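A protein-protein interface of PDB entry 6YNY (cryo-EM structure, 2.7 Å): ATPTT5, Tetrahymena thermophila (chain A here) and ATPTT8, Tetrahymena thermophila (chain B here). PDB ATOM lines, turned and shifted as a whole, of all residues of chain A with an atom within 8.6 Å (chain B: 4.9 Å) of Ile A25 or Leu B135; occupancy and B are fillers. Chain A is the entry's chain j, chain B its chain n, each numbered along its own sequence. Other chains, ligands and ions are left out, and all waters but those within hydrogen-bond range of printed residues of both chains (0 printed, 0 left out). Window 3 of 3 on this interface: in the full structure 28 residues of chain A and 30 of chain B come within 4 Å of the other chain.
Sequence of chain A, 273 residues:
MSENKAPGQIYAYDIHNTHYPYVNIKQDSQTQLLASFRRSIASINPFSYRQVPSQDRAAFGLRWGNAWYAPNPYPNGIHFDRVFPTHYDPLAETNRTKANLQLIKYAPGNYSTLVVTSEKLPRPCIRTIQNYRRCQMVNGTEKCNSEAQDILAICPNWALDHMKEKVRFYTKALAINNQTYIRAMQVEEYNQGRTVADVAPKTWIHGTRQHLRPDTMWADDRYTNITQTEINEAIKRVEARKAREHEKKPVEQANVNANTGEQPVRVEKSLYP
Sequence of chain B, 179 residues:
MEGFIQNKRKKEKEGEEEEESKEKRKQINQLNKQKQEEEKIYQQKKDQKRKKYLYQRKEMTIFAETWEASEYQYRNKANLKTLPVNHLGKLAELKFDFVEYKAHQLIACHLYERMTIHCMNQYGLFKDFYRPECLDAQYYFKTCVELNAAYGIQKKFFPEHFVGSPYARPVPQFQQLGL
NE2 of Gln A27 sits at hydrogen-bond distance from O of Tyr B130 (3.3 Å).
The side-chain hydroxyl (OH) of Tyr A69 sits at hydrogen-bond distance from the side-chain carboxylate (OD1) of Asp B136 (3.1 Å).
ND2 of Asn A72 is in hydrogen-bond range of OD2 of Asp B136 (3.1 Å).
The backbone carbonyl oxygen of Ile A25 lies within hydrogen-bond range of the side-chain amide nitrogen of Gln A27 (3.4 Å).
O of Arg A63 sits at hydrogen-bond distance from N of Ile A25, 2.9 Å away.
The backbone NH (N) of Tyr A69 sits at hydrogen-bond distance from the backbone carbonyl oxygen (O) of Leu A62, at 3.0 Å.
The guanidinium group of Arg B131 is in salt-bridge range of the side-chain carboxylate of Glu B133.
Ile A25 touches Tyr B130.
Arg B131 touches Ile A25.
Pro B132 touches Ile A25 (CD to O, 3.4 Å).
Ile A25 touches Leu B135.
Gln A27 touches Arg B131.
CB of Leu B135 touches OH of Tyr A69, at 3.5 Å.
Asp B136 touches Pro A71.
Tyr B139 touches Pro A71.
Asn A72 touches Tyr B139.
Of chain A, only Ile A25 and Tyr A69 come within 4 Å of Leu B135.
Pro B132 touches one residue of chain A.
Printed residues of chain B within 4 Å of Asn A72: Asp B136 and Tyr B139.
Of the printed residues of chain A, Tyr B130 touches Ile A25 and Gln A27.
Leu A62 touches none of the printed residues of chain B.
Phe B129 touches none of the printed residues of chain A.
The nearest printed residue of chain B that does not touch Gln A27 is Pro B132 (4.3 Å).
Of the 11 printed residues of chain B, 6 touch a printed residue of chain A.
Printed residues of chain B that touch a printed residue of chain A: Tyr B130, Arg B131, Pro B132, Leu B135, Asp B136 and Tyr B139.
Along chain B the printed residues that touch a printed residue of chain A span positions 130 to 139.
Among the printed residues, 12 pairs touch across the chains.
Among the printed residues, no Asp or Glu carboxylate lies within 4 Å of a Lys or Arg side-chain nitrogen of the other chain.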
ATOM      1  N   TYR A  22     -24.616  11.293 -13.361  1.00  0.00           N
ATOM      2  CA  TYR A  22     -24.196  11.576 -14.730  1.00  0.00           C
ATOM      3  C   TYR A  22     -25.344  12.265 -15.450  1.00  0.00           C
ATOM      4  O   TYR A  22     -26.153  11.636 -16.133  1.00  0.00           O
ATOM      5  CB  TYR A  22     -23.758  10.301 -15.430  1.00  0.00           C
ATOM      6  CG  TYR A  22     -22.349   9.900 -15.087  1.00  0.00           C
ATOM      7  CD1 TYR A  22     -22.034   9.412 -13.830  1.00  0.00           C
ATOM      8  CD2 TYR A  22     -21.332  10.015 -16.015  1.00  0.00           C
ATOM      9  CE1 TYR A  22     -20.750   9.050 -13.514  1.00  0.00           C
ATOM     10  CE2 TYR A  22     -20.049   9.656 -15.707  1.00  0.00           C
ATOM     11  CZ  TYR A  22     -19.764   9.173 -14.456  1.00  0.00           C
ATOM     12  OH  TYR A  22     -18.480   8.815 -14.154  1.00  0.00           O
ATOM     13  N   VAL A  23     -25.407  13.580 -15.291  1.00  0.00           N
ATOM     14  CA  VAL A  23     -26.463  14.399 -15.863  1.00  0.00           C
ATOM     15  C   VAL A  23     -25.951  14.983 -17.170  1.00  0.00           C
ATOM     16  O   VAL A  23     -25.077  15.857 -17.173  1.00  0.00           O
ATOM     17  CB  VAL A  23     -26.901  15.504 -14.896  1.00  0.00           C
ATOM     18  CG1 VAL A  23     -27.935  16.384 -15.543  1.00  0.00           C
ATOM     19  CG2 VAL A  23     -27.437  14.902 -13.624  1.00  0.00           C
ATOM     20  N   ASN A  24     -26.498  14.503 -18.280  1.00  0.00           N
ATOM     21  CA  ASN A  24     -26.193  15.018 -19.604  1.00  0.00           C
ATOM     22  C   ASN A  24     -27.457  15.618 -20.193  1.00  0.00           C
ATOM     23  O   ASN A  24     -28.517  14.988 -20.171  1.00  0.00           O
ATOM     24  CB  ASN A  24     -25.651  13.925 -20.521  1.00  0.00           C
ATOM     25  CG  ASN A  24     -24.893  14.481 -21.698  1.00  0.00           C
ATOM     26  OD1 ASN A  24     -25.473  15.070 -22.606  1.00  0.00           O
ATOM     27  ND2 ASN A  24     -23.588  14.285 -21.696  1.00  0.00           N
ATOM     28  N   ILE A  25     -27.338  16.837 -20.716  1.00  0.00           N
ATOM     29  CA  ILE A  25     -28.502  17.541 -21.233  1.00  0.00           C
ATOM     30  C   ILE A  25     -28.858  17.089 -22.640  1.00  0.00           C
ATOM     31  O   ILE A  25     -30.007  17.250 -23.063  1.00  0.00           O
ATOM     32  CB  ILE A  25     -28.249  19.055 -21.196  1.00  0.00           C
ATOM     33  CG1 ILE A  25     -27.715  19.472 -19.827  1.00  0.00           C
ATOM     34  CG2 ILE A  25     -29.508  19.813 -21.492  1.00  0.00           C
ATOM     35  CD1 ILE A  25     -28.574  19.063 -18.686  1.00  0.00           C
ATOM     36  N   LYS A  26     -27.905  16.529 -23.376  1.00  0.00           N
ATOM     37  CA  LYS A  26     -28.164  16.076 -24.733  1.00  0.00           C
ATOM     38  C   LYS A  26     -29.076  14.858 -24.695  1.00  0.00           C
ATOM     39  O   LYS A  26     -28.715  13.820 -24.132  1.00  0.00           O
ATOM     40  CB  LYS A  26     -26.849  15.754 -25.434  1.00  0.00           C
ATOM     41  CG  LYS A  26     -26.867  16.003 -26.918  1.00  0.00           C
ATOM     42  CD  LYS A  26     -25.492  15.839 -27.511  1.00  0.00           C
ATOM     43  CE  LYS A  26     -25.473  16.214 -28.973  1.00  0.00           C
ATOM     44  NZ  LYS A  26     -26.305  15.307 -29.797  1.00  0.00           N
ATOM     45  N   GLN A  27     -30.255  14.985 -25.294  1.00  0.00           N
ATOM     46  CA  GLN A  27     -31.269  13.936 -25.248  1.00  0.00           C
ATOM     47  C   GLN A  27     -31.197  13.072 -26.504  1.00  0.00           C
ATOM     48  O   GLN A  27     -32.083  13.075 -27.358  1.00  0.00           O
ATOM     49  CB  GLN A  27     -32.654  14.551 -25.073  1.00  0.00           C
ATOM     50  CG  GLN A  27     -32.836  15.301 -23.777  1.00  0.00           C
ATOM     51  CD  GLN A  27     -32.645  14.425 -22.564  1.00  0.00           C
ATOM     52  OE1 GLN A  27     -33.064  13.269 -22.544  1.00  0.00           O
ATOM     53  NE2 GLN A  27     -32.004  14.969 -21.543  1.00  0.00           N
ATOM     54  N   ASP A  28     -30.104  12.326 -26.604  1.00  0.00           N
ATOM     55  CA  ASP A  28     -29.949  11.297 -27.618  1.00  0.00           C
ATOM     56  C   ASP A  28     -29.729   9.956 -26.933  1.00  0.00           C
ATOM     57  O   ASP A  28     -29.140   9.883 -25.851  1.00  0.00           O
ATOM     58  CB  ASP A  28     -28.791  11.605 -28.576  1.00  0.00           C
ATOM     59  CG  ASP A  28     -27.446  11.630 -27.885  1.00  0.00           C
ATOM     60  OD1 ASP A  28     -26.938  10.549 -27.526  1.00  0.00           O
ATOM     61  OD2 ASP A  28     -26.889  12.732 -27.711  1.00  0.00           O
ATOM     62  N   THR A  31     -26.305   8.970 -25.770  1.00  0.00           N
ATOM     63  CA  THR A  31     -25.774   9.707 -24.632  1.00  0.00           C
ATOM     64  C   THR A  31     -26.409   9.263 -23.323  1.00  0.00           C
ATOM     65  O   THR A  31     -25.708   9.080 -22.322  1.00  0.00           O
ATOM     66  CB  THR A  31     -25.988  11.202 -24.850  1.00  0.00           C
ATOM     67  OG1 THR A  31     -25.231  11.635 -25.984  1.00  0.00           O
ATOM     68  CG2 THR A  31     -25.561  11.983 -23.639  1.00  0.00           C
ATOM     69  N   GLN A  32     -27.731   9.095 -23.303  1.00  0.00           N
ATOM     70  CA  GLN A  32     -28.410   8.758 -22.060  1.00  0.00           C
ATOM     71  C   GLN A  32     -28.154   7.316 -21.643  1.00  0.00           C
ATOM     72  O   GLN A  32     -28.084   7.026 -20.443  1.00  0.00           O
ATOM     73  CB  GLN A  32     -29.905   9.016 -22.201  1.00  0.00           C
ATOM     74  CG  GLN A  32     -30.247  10.474 -22.408  1.00  0.00           C
ATOM     75  CD  GLN A  32     -29.788  11.343 -21.259  1.00  0.00           C
ATOM     76  OE1 GLN A  32     -29.813  10.928 -20.102  1.00  0.00           O
ATOM     77  NE2 GLN A  32     -29.356  12.553 -21.572  1.00  0.00           N
ATOM     78  N   ALA A  35     -24.842   7.280 -20.061  1.00  0.00           N
ATOM     79  CA  ALA A  35     -24.925   7.926 -18.758  1.00  0.00           C
ATOM     80  C   ALA A  35     -25.533   6.996 -17.721  1.00  0.00           C
ATOM     81  O   ALA A  35     -25.060   6.935 -16.580  1.00  0.00           O
ATOM     82  CB  ALA A  35     -25.738   9.210 -18.866  1.00  0.00           C
ATOM     83  N   TYR A  49     -16.181  11.333 -12.807  1.00  0.00           N
ATOM     84  CA  TYR A  49     -16.032  12.744 -12.501  1.00  0.00           C
ATOM     85  C   TYR A  49     -17.254  13.230 -11.742  1.00  0.00           C
ATOM     86  O   TYR A  49     -18.388  12.887 -12.084  1.00  0.00           O
ATOM     87  CB  TYR A  49     -15.834  13.579 -13.772  1.00  0.00           C
ATOM     88  CG  TYR A  49     -16.996  13.561 -14.733  1.00  0.00           C
ATOM     89  CD1 TYR A  49     -18.011  14.497 -14.638  1.00  0.00           C
ATOM     90  CD2 TYR A  49     -17.070  12.623 -15.744  1.00  0.00           C
ATOM     91  CE1 TYR A  49     -19.065  14.490 -15.511  1.00  0.00           C
ATOM     92  CE2 TYR A  49     -18.122  12.610 -16.624  1.00  0.00           C
ATOM     93  CZ  TYR A  49     -19.117  13.548 -16.504  1.00  0.00           C
ATOM     94  OH  TYR A  49     -20.171  13.537 -17.379  1.00  0.00           O
ATOM     95  N   GLN A  51     -20.106  15.758 -10.326  1.00  0.00           N
ATOM     96  CA  GLN A  51     -20.913  16.902 -10.710  1.00  0.00           C
ATOM     97  C   GLN A  51     -21.578  17.557  -9.512  1.00  0.00           C
ATOM     98  O   GLN A  51     -22.251  18.582  -9.677  1.00  0.00           O
ATOM     99  CB  GLN A  51     -21.970  16.488 -11.739  1.00  0.00           C
ATOM    100  CG  GLN A  51     -21.399  16.280 -13.122  1.00  0.00           C
ATOM    101  CD  GLN A  51     -22.431  15.858 -14.134  1.00  0.00           C
ATOM    102  OE1 GLN A  51     -22.883  14.719 -14.135  1.00  0.00           O
ATOM    103  NE2 GLN A  51     -22.797  16.770 -15.015  1.00  0.00           N
ATOM    104  N   GLY A  61     -19.614  20.927 -14.085  1.00  0.00           N
ATOM    105  CA  GLY A  61     -20.974  21.338 -14.343  1.00  0.00           C
ATOM    106  C   GLY A  61     -21.731  20.313 -15.154  1.00  0.00           C
ATOM    107  O   GLY A  61     -21.339  19.151 -15.267  1.00  0.00           O
ATOM    108  N   LEU A  62     -22.838  20.762 -15.733  1.00  0.00           N
ATOM    109  CA  LEU A  62     -23.664  19.881 -16.542  1.00  0.00           C
ATOM    110  C   LEU A  62     -22.978  19.592 -17.868  1.00  0.00           C
ATOM    111  O   LEU A  62     -22.344  20.466 -18.463  1.00  0.00           O
ATOM    112  CB  LEU A  62     -25.034  20.505 -16.781  1.00  0.00           C
ATOM    113  CG  LEU A  62     -25.808  20.917 -15.534  1.00  0.00           C
ATOM    114  CD1 LEU A  62     -27.097  21.576 -15.929  1.00  0.00           C
ATOM    115  CD2 LEU A  62     -26.078  19.727 -14.647  1.00  0.00           C
ATOM    116  N   ARG A  63     -23.110  18.355 -18.328  1.00  0.00           N
ATOM    117  CA  ARG A  63     -22.452  17.891 -19.537  1.00  0.00           C
ATOM    118  C   ARG A  63     -23.398  17.990 -20.726  1.00  0.00           C
ATOM    119  O   ARG A  63     -24.606  17.773 -20.594  1.00  0.00           O
ATOM    120  CB  ARG A  63     -21.982  16.448 -19.359  1.00  0.00           C
ATOM    121  CG  ARG A  63     -20.915  15.996 -20.326  1.00  0.00           C
ATOM    122  CD  ARG A  63     -19.580  16.578 -19.963  1.00  0.00           C
ATOM    123  NE  ARG A  63     -18.506  16.110 -20.829  1.00  0.00           N
ATOM    124  CZ  ARG A  63     -17.756  15.042 -20.595  1.00  0.00           C
ATOM    125  NH1 ARG A  63     -17.946  14.302 -19.517  1.00  0.00           N
ATOM    126  NH2 ARG A  63     -16.806  14.715 -21.451  1.00  0.00           N
ATOM    127  N   TRP A  64     -22.840  18.330 -21.883  1.00  0.00           N
ATOM    128  CA  TRP A  64     -23.546  18.333 -23.160  1.00  0.00           C
ATOM    129  C   TRP A  64     -22.769  17.405 -24.084  1.00  0.00           C
ATOM    130  O   TRP A  64     -21.824  17.826 -24.754  1.00  0.00           O
ATOM    131  CB  TRP A  64     -23.668  19.727 -23.747  1.00  0.00           C
ATOM    132  CG  TRP A  64     -24.272  19.725 -25.106  1.00  0.00           C
ATOM    133  CD1 TRP A  64     -23.611  19.711 -26.294  1.00  0.00           C
ATOM    134  CD2 TRP A  64     -25.664  19.719 -25.422  1.00  0.00           C
ATOM    135  NE1 TRP A  64     -24.503  19.701 -27.331  1.00  0.00           N
ATOM    136  CE2 TRP A  64     -25.773  19.706 -26.822  1.00  0.00           C
ATOM    137  CE3 TRP A  64     -26.828  19.726 -24.657  1.00  0.00           C
ATOM    138  CZ2 TRP A  64     -26.999  19.701 -27.470  1.00  0.00           C
ATOM    139  CZ3 TRP A  64     -28.041  19.722 -25.301  1.00  0.00           C
ATOM    140  CH2 TRP A  64     -28.119  19.708 -26.693  1.00  0.00           C
ATOM    141  N   GLY A  65     -23.169  16.147 -24.120  1.00  0.00           N
ATOM    142  CA  GLY A  65     -22.415  15.167 -24.875  1.00  0.00           C
ATOM    143  C   GLY A  65     -21.019  15.038 -24.306  1.00  0.00           C
ATOM    144  O   GLY A  65     -20.831  14.752 -23.119  1.00  0.00           O
ATOM    145  N   ALA A  67     -18.942  17.703 -24.638  1.00  0.00           N
ATOM    146  CA  ALA A  67     -18.670  19.071 -24.235  1.00  0.00           C
ATOM    147  C   ALA A  67     -19.481  19.412 -22.986  1.00  0.00           C
ATOM    148  O   ALA A  67     -20.040  18.535 -22.323  1.00  0.00           O
ATOM    149  CB  ALA A  67     -18.966  20.023 -25.388  1.00  0.00           C
ATOM    150  N   TRP A  68     -19.542  20.694 -22.647  1.00  0.00           N
ATOM    151  CA  TRP A  68     -20.239  21.170 -21.465  1.00  0.00           C
ATOM    152  C   TRP A  68     -21.446  22.009 -21.858  1.00  0.00           C
ATOM    153  O   TRP A  68     -21.550  22.508 -22.981  1.00  0.00           O
ATOM    154  CB  TRP A  68     -19.294  21.980 -20.576  1.00  0.00           C
ATOM    155  CG  TRP A  68     -18.103  21.195 -20.187  1.00  0.00           C
ATOM    156  CD1 TRP A  68     -16.850  21.305 -20.697  1.00  0.00           C
ATOM    157  CD2 TRP A  68     -18.052  20.150 -19.216  1.00  0.00           C
ATOM    158  NE1 TRP A  68     -16.018  20.397 -20.102  1.00  0.00           N
ATOM    159  CE2 TRP A  68     -16.733  19.674 -19.187  1.00  0.00           C
ATOM    160  CE3 TRP A  68     -18.993  19.573 -18.367  1.00  0.00           C
ATOM    161  CZ2 TRP A  68     -16.333  18.650 -18.344  1.00  0.00           C
ATOM    162  CZ3 TRP A  68     -18.594  18.559 -17.534  1.00  0.00           C
ATOM    163  CH2 TRP A  68     -17.278  18.107 -17.526  1.00  0.00           C
ATOM    164  N   TYR A  69     -22.365  22.154 -20.911  1.00  0.00           N
ATOM    165  CA  TYR A  69     -23.648  22.795 -21.145  1.00  0.00           C
ATOM    166  C   TYR A  69     -23.697  24.170 -20.502  1.00  0.00           C
ATOM    167  O   TYR A  69     -23.146  24.384 -19.419  1.00  0.00           O
ATOM    168  CB  TYR A  69     -24.795  21.945 -20.598  1.00  0.00           C
ATOM    169  CG  TYR A  69     -26.113  22.679 -20.532  1.00  0.00           C
ATOM    170  CD1 TYR A  69     -26.916  22.802 -21.652  1.00  0.00           C
ATOM    171  CD2 TYR A  69     -26.547  23.258 -19.352  1.00  0.00           C
ATOM    172  CE1 TYR A  69     -28.110  23.477 -21.597  1.00  0.00           C
ATOM    173  CE2 TYR A  69     -27.740  23.932 -19.289  1.00  0.00           C
ATOM    174  CZ  TYR A  69     -28.520  24.038 -20.413  1.00  0.00           C
ATOM    175  OH  TYR A  69     -29.715  24.711 -20.358  1.00  0.00           O
ATOM    176  N   ALA A  70     -24.368  25.096 -21.184  1.00  0.00           N
ATOM    177  CA  ALA A  70     -24.723  26.382 -20.644  1.00  0.00           C
ATOM    178  C   ALA A  70     -25.964  26.826 -21.399  1.00  0.00           C
ATOM    179  O   ALA A  70     -26.029  26.637 -22.621  1.00  0.00           O
ATOM    180  CB  ALA A  70     -23.615  27.420 -20.791  1.00  0.00           C
ATOM    181  N   PRO A  71     -26.959  27.391 -20.720  1.00  0.00           N
ATOM    182  CA  PRO A  71     -28.170  27.815 -21.424  1.00  0.00           C
ATOM    183  C   PRO A  71     -27.861  28.835 -22.506  1.00  0.00           C
ATOM    184  O   PRO A  71     -26.823  29.499 -22.496  1.00  0.00           O
ATOM    185  CB  PRO A  71     -29.029  28.429 -20.314  1.00  0.00           C
ATOM    186  CG  PRO A  71     -28.497  27.886 -19.063  1.00  0.00           C
ATOM    187  CD  PRO A  71     -27.046  27.664 -19.279  1.00  0.00           C
ATOM    188  N   ASN A  72     -28.779  28.951 -23.452  1.00  0.00           N
ATOM    189  CA  ASN A  72     -28.673  30.011 -24.438  1.00  0.00           C
ATOM    190  C   ASN A  72     -28.766  31.358 -23.731  1.00  0.00           C
ATOM    191  O   ASN A  72     -29.664  31.553 -22.903  1.00  0.00           O
ATOM    192  CB  ASN A  72     -29.770  29.906 -25.494  1.00  0.00           C
ATOM    193  CG  ASN A  72     -29.424  28.947 -26.602  1.00  0.00           C
ATOM    194  OD1 ASN A  72     -28.512  29.194 -27.388  1.00  0.00           O
ATOM    195  ND2 ASN A  72     -30.167  27.854 -26.688  1.00  0.00           N
ATOM    196  N   PHE B 129     -36.610  16.767 -16.315  1.00  0.00           N
ATOM    197  CA  PHE B 129     -36.697  18.190 -16.588  1.00  0.00           C
ATOM    198  C   PHE B 129     -35.390  18.748 -17.124  1.00  0.00           C
ATOM    199  O   PHE B 129     -35.388  19.837 -17.706  1.00  0.00           O
ATOM    200  CB  PHE B 129     -37.092  18.918 -15.307  1.00  0.00           C
ATOM    201  CG  PHE B 129     -37.243  20.392 -15.464  1.00  0.00           C
ATOM    202  CD1 PHE B 129     -38.391  20.928 -16.002  1.00  0.00           C
ATOM    203  CD2 PHE B 129     -36.244  21.244 -15.048  1.00  0.00           C
ATOM    204  CE1 PHE B 129     -38.533  22.285 -16.137  1.00  0.00           C
ATOM    205  CE2 PHE B 129     -36.382  22.600 -15.182  1.00  0.00           C
ATOM    206  CZ  PHE B 129     -37.528  23.122 -15.727  1.00  0.00           C
ATOM    207  N   TYR B 130     -34.288  18.020 -16.955  1.00  0.00           N
ATOM    208  CA  TYR B 130     -32.973  18.487 -17.381  1.00  0.00           C
ATOM    209  C   TYR B 130     -32.779  18.161 -18.860  1.00  0.00           C
ATOM    210  O   TYR B 130     -31.984  17.309 -19.260  1.00  0.00           O
ATOM    211  CB  TYR B 130     -31.887  17.884 -16.505  1.00  0.00           C
ATOM    212  CG  TYR B 130     -31.733  18.621 -15.203  1.00  0.00           C
ATOM    213  CD1 TYR B 130     -30.763  19.596 -15.051  1.00  0.00           C
ATOM    214  CD2 TYR B 130     -32.575  18.367 -14.137  1.00  0.00           C
ATOM    215  CE1 TYR B 130     -30.626  20.281 -13.872  1.00  0.00           C
ATOM    216  CE2 TYR B 130     -32.445  19.049 -12.954  1.00  0.00           C
ATOM    217  CZ  TYR B 130     -31.470  20.007 -12.826  1.00  0.00           C
ATOM    218  OH  TYR B 130     -31.334  20.693 -11.645  1.00  0.00           O
ATOM    219  N   ARG B 131     -33.538  18.876 -19.677  1.00  0.00           N
ATOM    220  CA  ARG B 131     -33.444  18.851 -21.124  1.00  0.00           C
ATOM    221  C   ARG B 131     -33.438  20.282 -21.635  1.00  0.00           C
ATOM    222  O   ARG B 131     -33.998  21.174 -20.994  1.00  0.00           O
ATOM    223  CB  ARG B 131     -34.613  18.066 -21.736  1.00  0.00           C
ATOM    224  CG  ARG B 131     -35.963  18.660 -21.464  1.00  0.00           C
ATOM    225  CD  ARG B 131     -37.061  17.620 -21.509  1.00  0.00           C
ATOM    226  NE  ARG B 131     -37.041  16.824 -22.730  1.00  0.00           N
ATOM    227  CZ  ARG B 131     -36.996  15.496 -22.772  1.00  0.00           C
ATOM    228  NH1 ARG B 131     -36.977  14.775 -21.660  1.00  0.00           N
ATOM    229  NH2 ARG B 131     -36.981  14.881 -23.943  1.00  0.00           N
ATOM    230  N   PRO B 132     -32.808  20.533 -22.784  1.00  0.00           N
ATOM    231  CA  PRO B 132     -32.519  21.928 -23.155  1.00  0.00           C
ATOM    232  C   PRO B 132     -33.752  22.795 -23.312  1.00  0.00           C
ATOM    233  O   PRO B 132     -33.708  23.986 -22.980  1.00  0.00           O
ATOM    234  CB  PRO B 132     -31.749  21.778 -24.474  1.00  0.00           C
ATOM    235  CG  PRO B 132     -32.168  20.482 -25.012  1.00  0.00           C
ATOM    236  CD  PRO B 132     -32.413  19.593 -23.844  1.00  0.00           C
ATOM    237  N   GLU B 133     -34.856  22.240 -23.811  1.00  0.00           N
ATOM    238  CA  GLU B 133     -36.047  23.052 -24.027  1.00  0.00           C
ATOM    239  C   GLU B 133     -36.646  23.541 -22.717  1.00  0.00           C
ATOM    240  O   GLU B 133     -37.240  24.624 -22.678  1.00  0.00           O
ATOM    241  CB  GLU B 133     -37.092  22.269 -24.821  1.00  0.00           C
ATOM    242  CG  GLU B 133     -37.429  20.898 -24.261  1.00  0.00           C
ATOM    243  CD  GLU B 133     -36.568  19.796 -24.846  1.00  0.00           C
ATOM    244  OE1 GLU B 133     -35.578  20.112 -25.538  1.00  0.00           O
ATOM    245  OE2 GLU B 133     -36.882  18.611 -24.613  1.00  0.00           O
ATOM    246  N   CYS B 134     -36.499  22.773 -21.642  1.00  0.00           N
ATOM    247  CA  CYS B 134     -37.112  23.127 -20.370  1.00  0.00           C
ATOM    248  C   CYS B 134     -36.199  23.964 -19.486  1.00  0.00           C
ATOM    249  O   CYS B 134     -36.691  24.810 -18.733  1.00  0.00           O
ATOM    250  CB  CYS B 134     -37.521  21.859 -19.617  1.00  0.00           C
ATOM    251  SG  CYS B 134     -38.369  20.637 -20.625  1.00  0.00           S
ATOM    252  N   LEU B 135     -34.885  23.745 -19.552  1.00  0.00           N
ATOM    253  CA  LEU B 135     -33.971  24.531 -18.734  1.00  0.00           C
ATOM    254  C   LEU B 135     -33.816  25.949 -19.265  1.00  0.00           C
ATOM    255  O   LEU B 135     -33.601  26.879 -18.481  1.00  0.00           O
ATOM    256  CB  LEU B 135     -32.610  23.847 -18.659  1.00  0.00           C
ATOM    257  CG  LEU B 135     -32.555  22.515 -17.919  1.00  0.00           C
ATOM    258  CD1 LEU B 135     -31.172  21.938 -18.008  1.00  0.00           C
ATOM    259  CD2 LEU B 135     -32.958  22.673 -16.472  1.00  0.00           C
ATOM    260  N   ASP B 136     -33.906  26.136 -20.580  1.00  0.00           N
ATOM    261  CA  ASP B 136     -33.821  27.482 -21.131  1.00  0.00           C
ATOM    262  C   ASP B 136     -35.043  28.310 -20.764  1.00  0.00           C
ATOM    263  O   ASP B 136     -34.936  29.529 -20.600  1.00  0.00           O
ATOM    264  CB  ASP B 136     -33.655  27.426 -22.645  1.00  0.00           C
ATOM    265  CG  ASP B 136     -32.275  26.974 -23.066  1.00  0.00           C
ATOM    266  OD1 ASP B 136     -31.509  26.499 -22.201  1.00  0.00           O
ATOM    267  OD2 ASP B 136     -31.949  27.102 -24.264  1.00  0.00           O
ATOM    268  N   ALA B 137     -36.205  27.673 -20.633  1.00  0.00           N
ATOM    269  CA  ALA B 137     -37.395  28.396 -20.208  1.00  0.00           C
ATOM    270  C   ALA B 137     -37.273  28.834 -18.757  1.00  0.00           C
ATOM    271  O   ALA B 137     -37.662  29.951 -18.401  1.00  0.00           O
ATOM    272  CB  ALA B 137     -38.632  27.524 -20.405  1.00  0.00           C
ATOM    273  N   GLN B 138     -36.735  27.962 -17.904  1.00  0.00           N
ATOM    274  CA  GLN B 138     -36.513  28.323 -16.513  1.00  0.00           C
ATOM    275  C   GLN B 138     -35.468  29.422 -16.388  1.00  0.00           C
ATOM    276  O   GLN B 138     -35.574  30.292 -15.517  1.00  0.00           O
ATOM    277  CB  GLN B 138     -36.090  27.085 -15.729  1.00  0.00           C
ATOM    278  CG  GLN B 138     -36.043  27.270 -14.238  1.00  0.00           C
ATOM    279  CD  GLN B 138     -35.430  26.084 -13.533  1.00  0.00           C
ATOM    280  OE1 GLN B 138     -34.836  25.213 -14.163  1.00  0.00           O
ATOM    281  NE2 GLN B 138     -35.569  26.043 -12.218  1.00  0.00           N
ATOM    282  N   TYR B 139     -34.445  29.397 -17.244  1.00  0.00           N
ATOM    283  CA  TYR B 139     -33.410  30.421 -17.188  1.00  0.00           C
ATOM    284  C   TYR B 139     -33.917  31.748 -17.734  1.00  0.00           C
ATOM    285  O   TYR B 139     -33.623  32.808 -17.171  1.00  0.00           O
ATOM    286  CB  TYR B 139     -32.177  29.955 -17.958  1.00  0.00           C
ATOM    287  CG  TYR B 139     -31.103  31.003 -18.082  1.00  0.00           C
ATOM    288  CD1 TYR B 139     -30.308  31.340 -17.002  1.00  0.00           C
ATOM    289  CD2 TYR B 139     -30.882  31.655 -19.281  1.00  0.00           C
ATOM    290  CE1 TYR B 139     -29.332  32.296 -17.111  1.00  0.00           C
ATOM    291  CE2 TYR B 139     -29.906  32.613 -19.399  1.00  0.00           C
ATOM    292  CZ  TYR B 139     -29.134  32.929 -18.310  1.00  0.00           C
ATOM    293  OH  TYR B 139     -28.157  33.886 -18.425  1.00  0.00           O
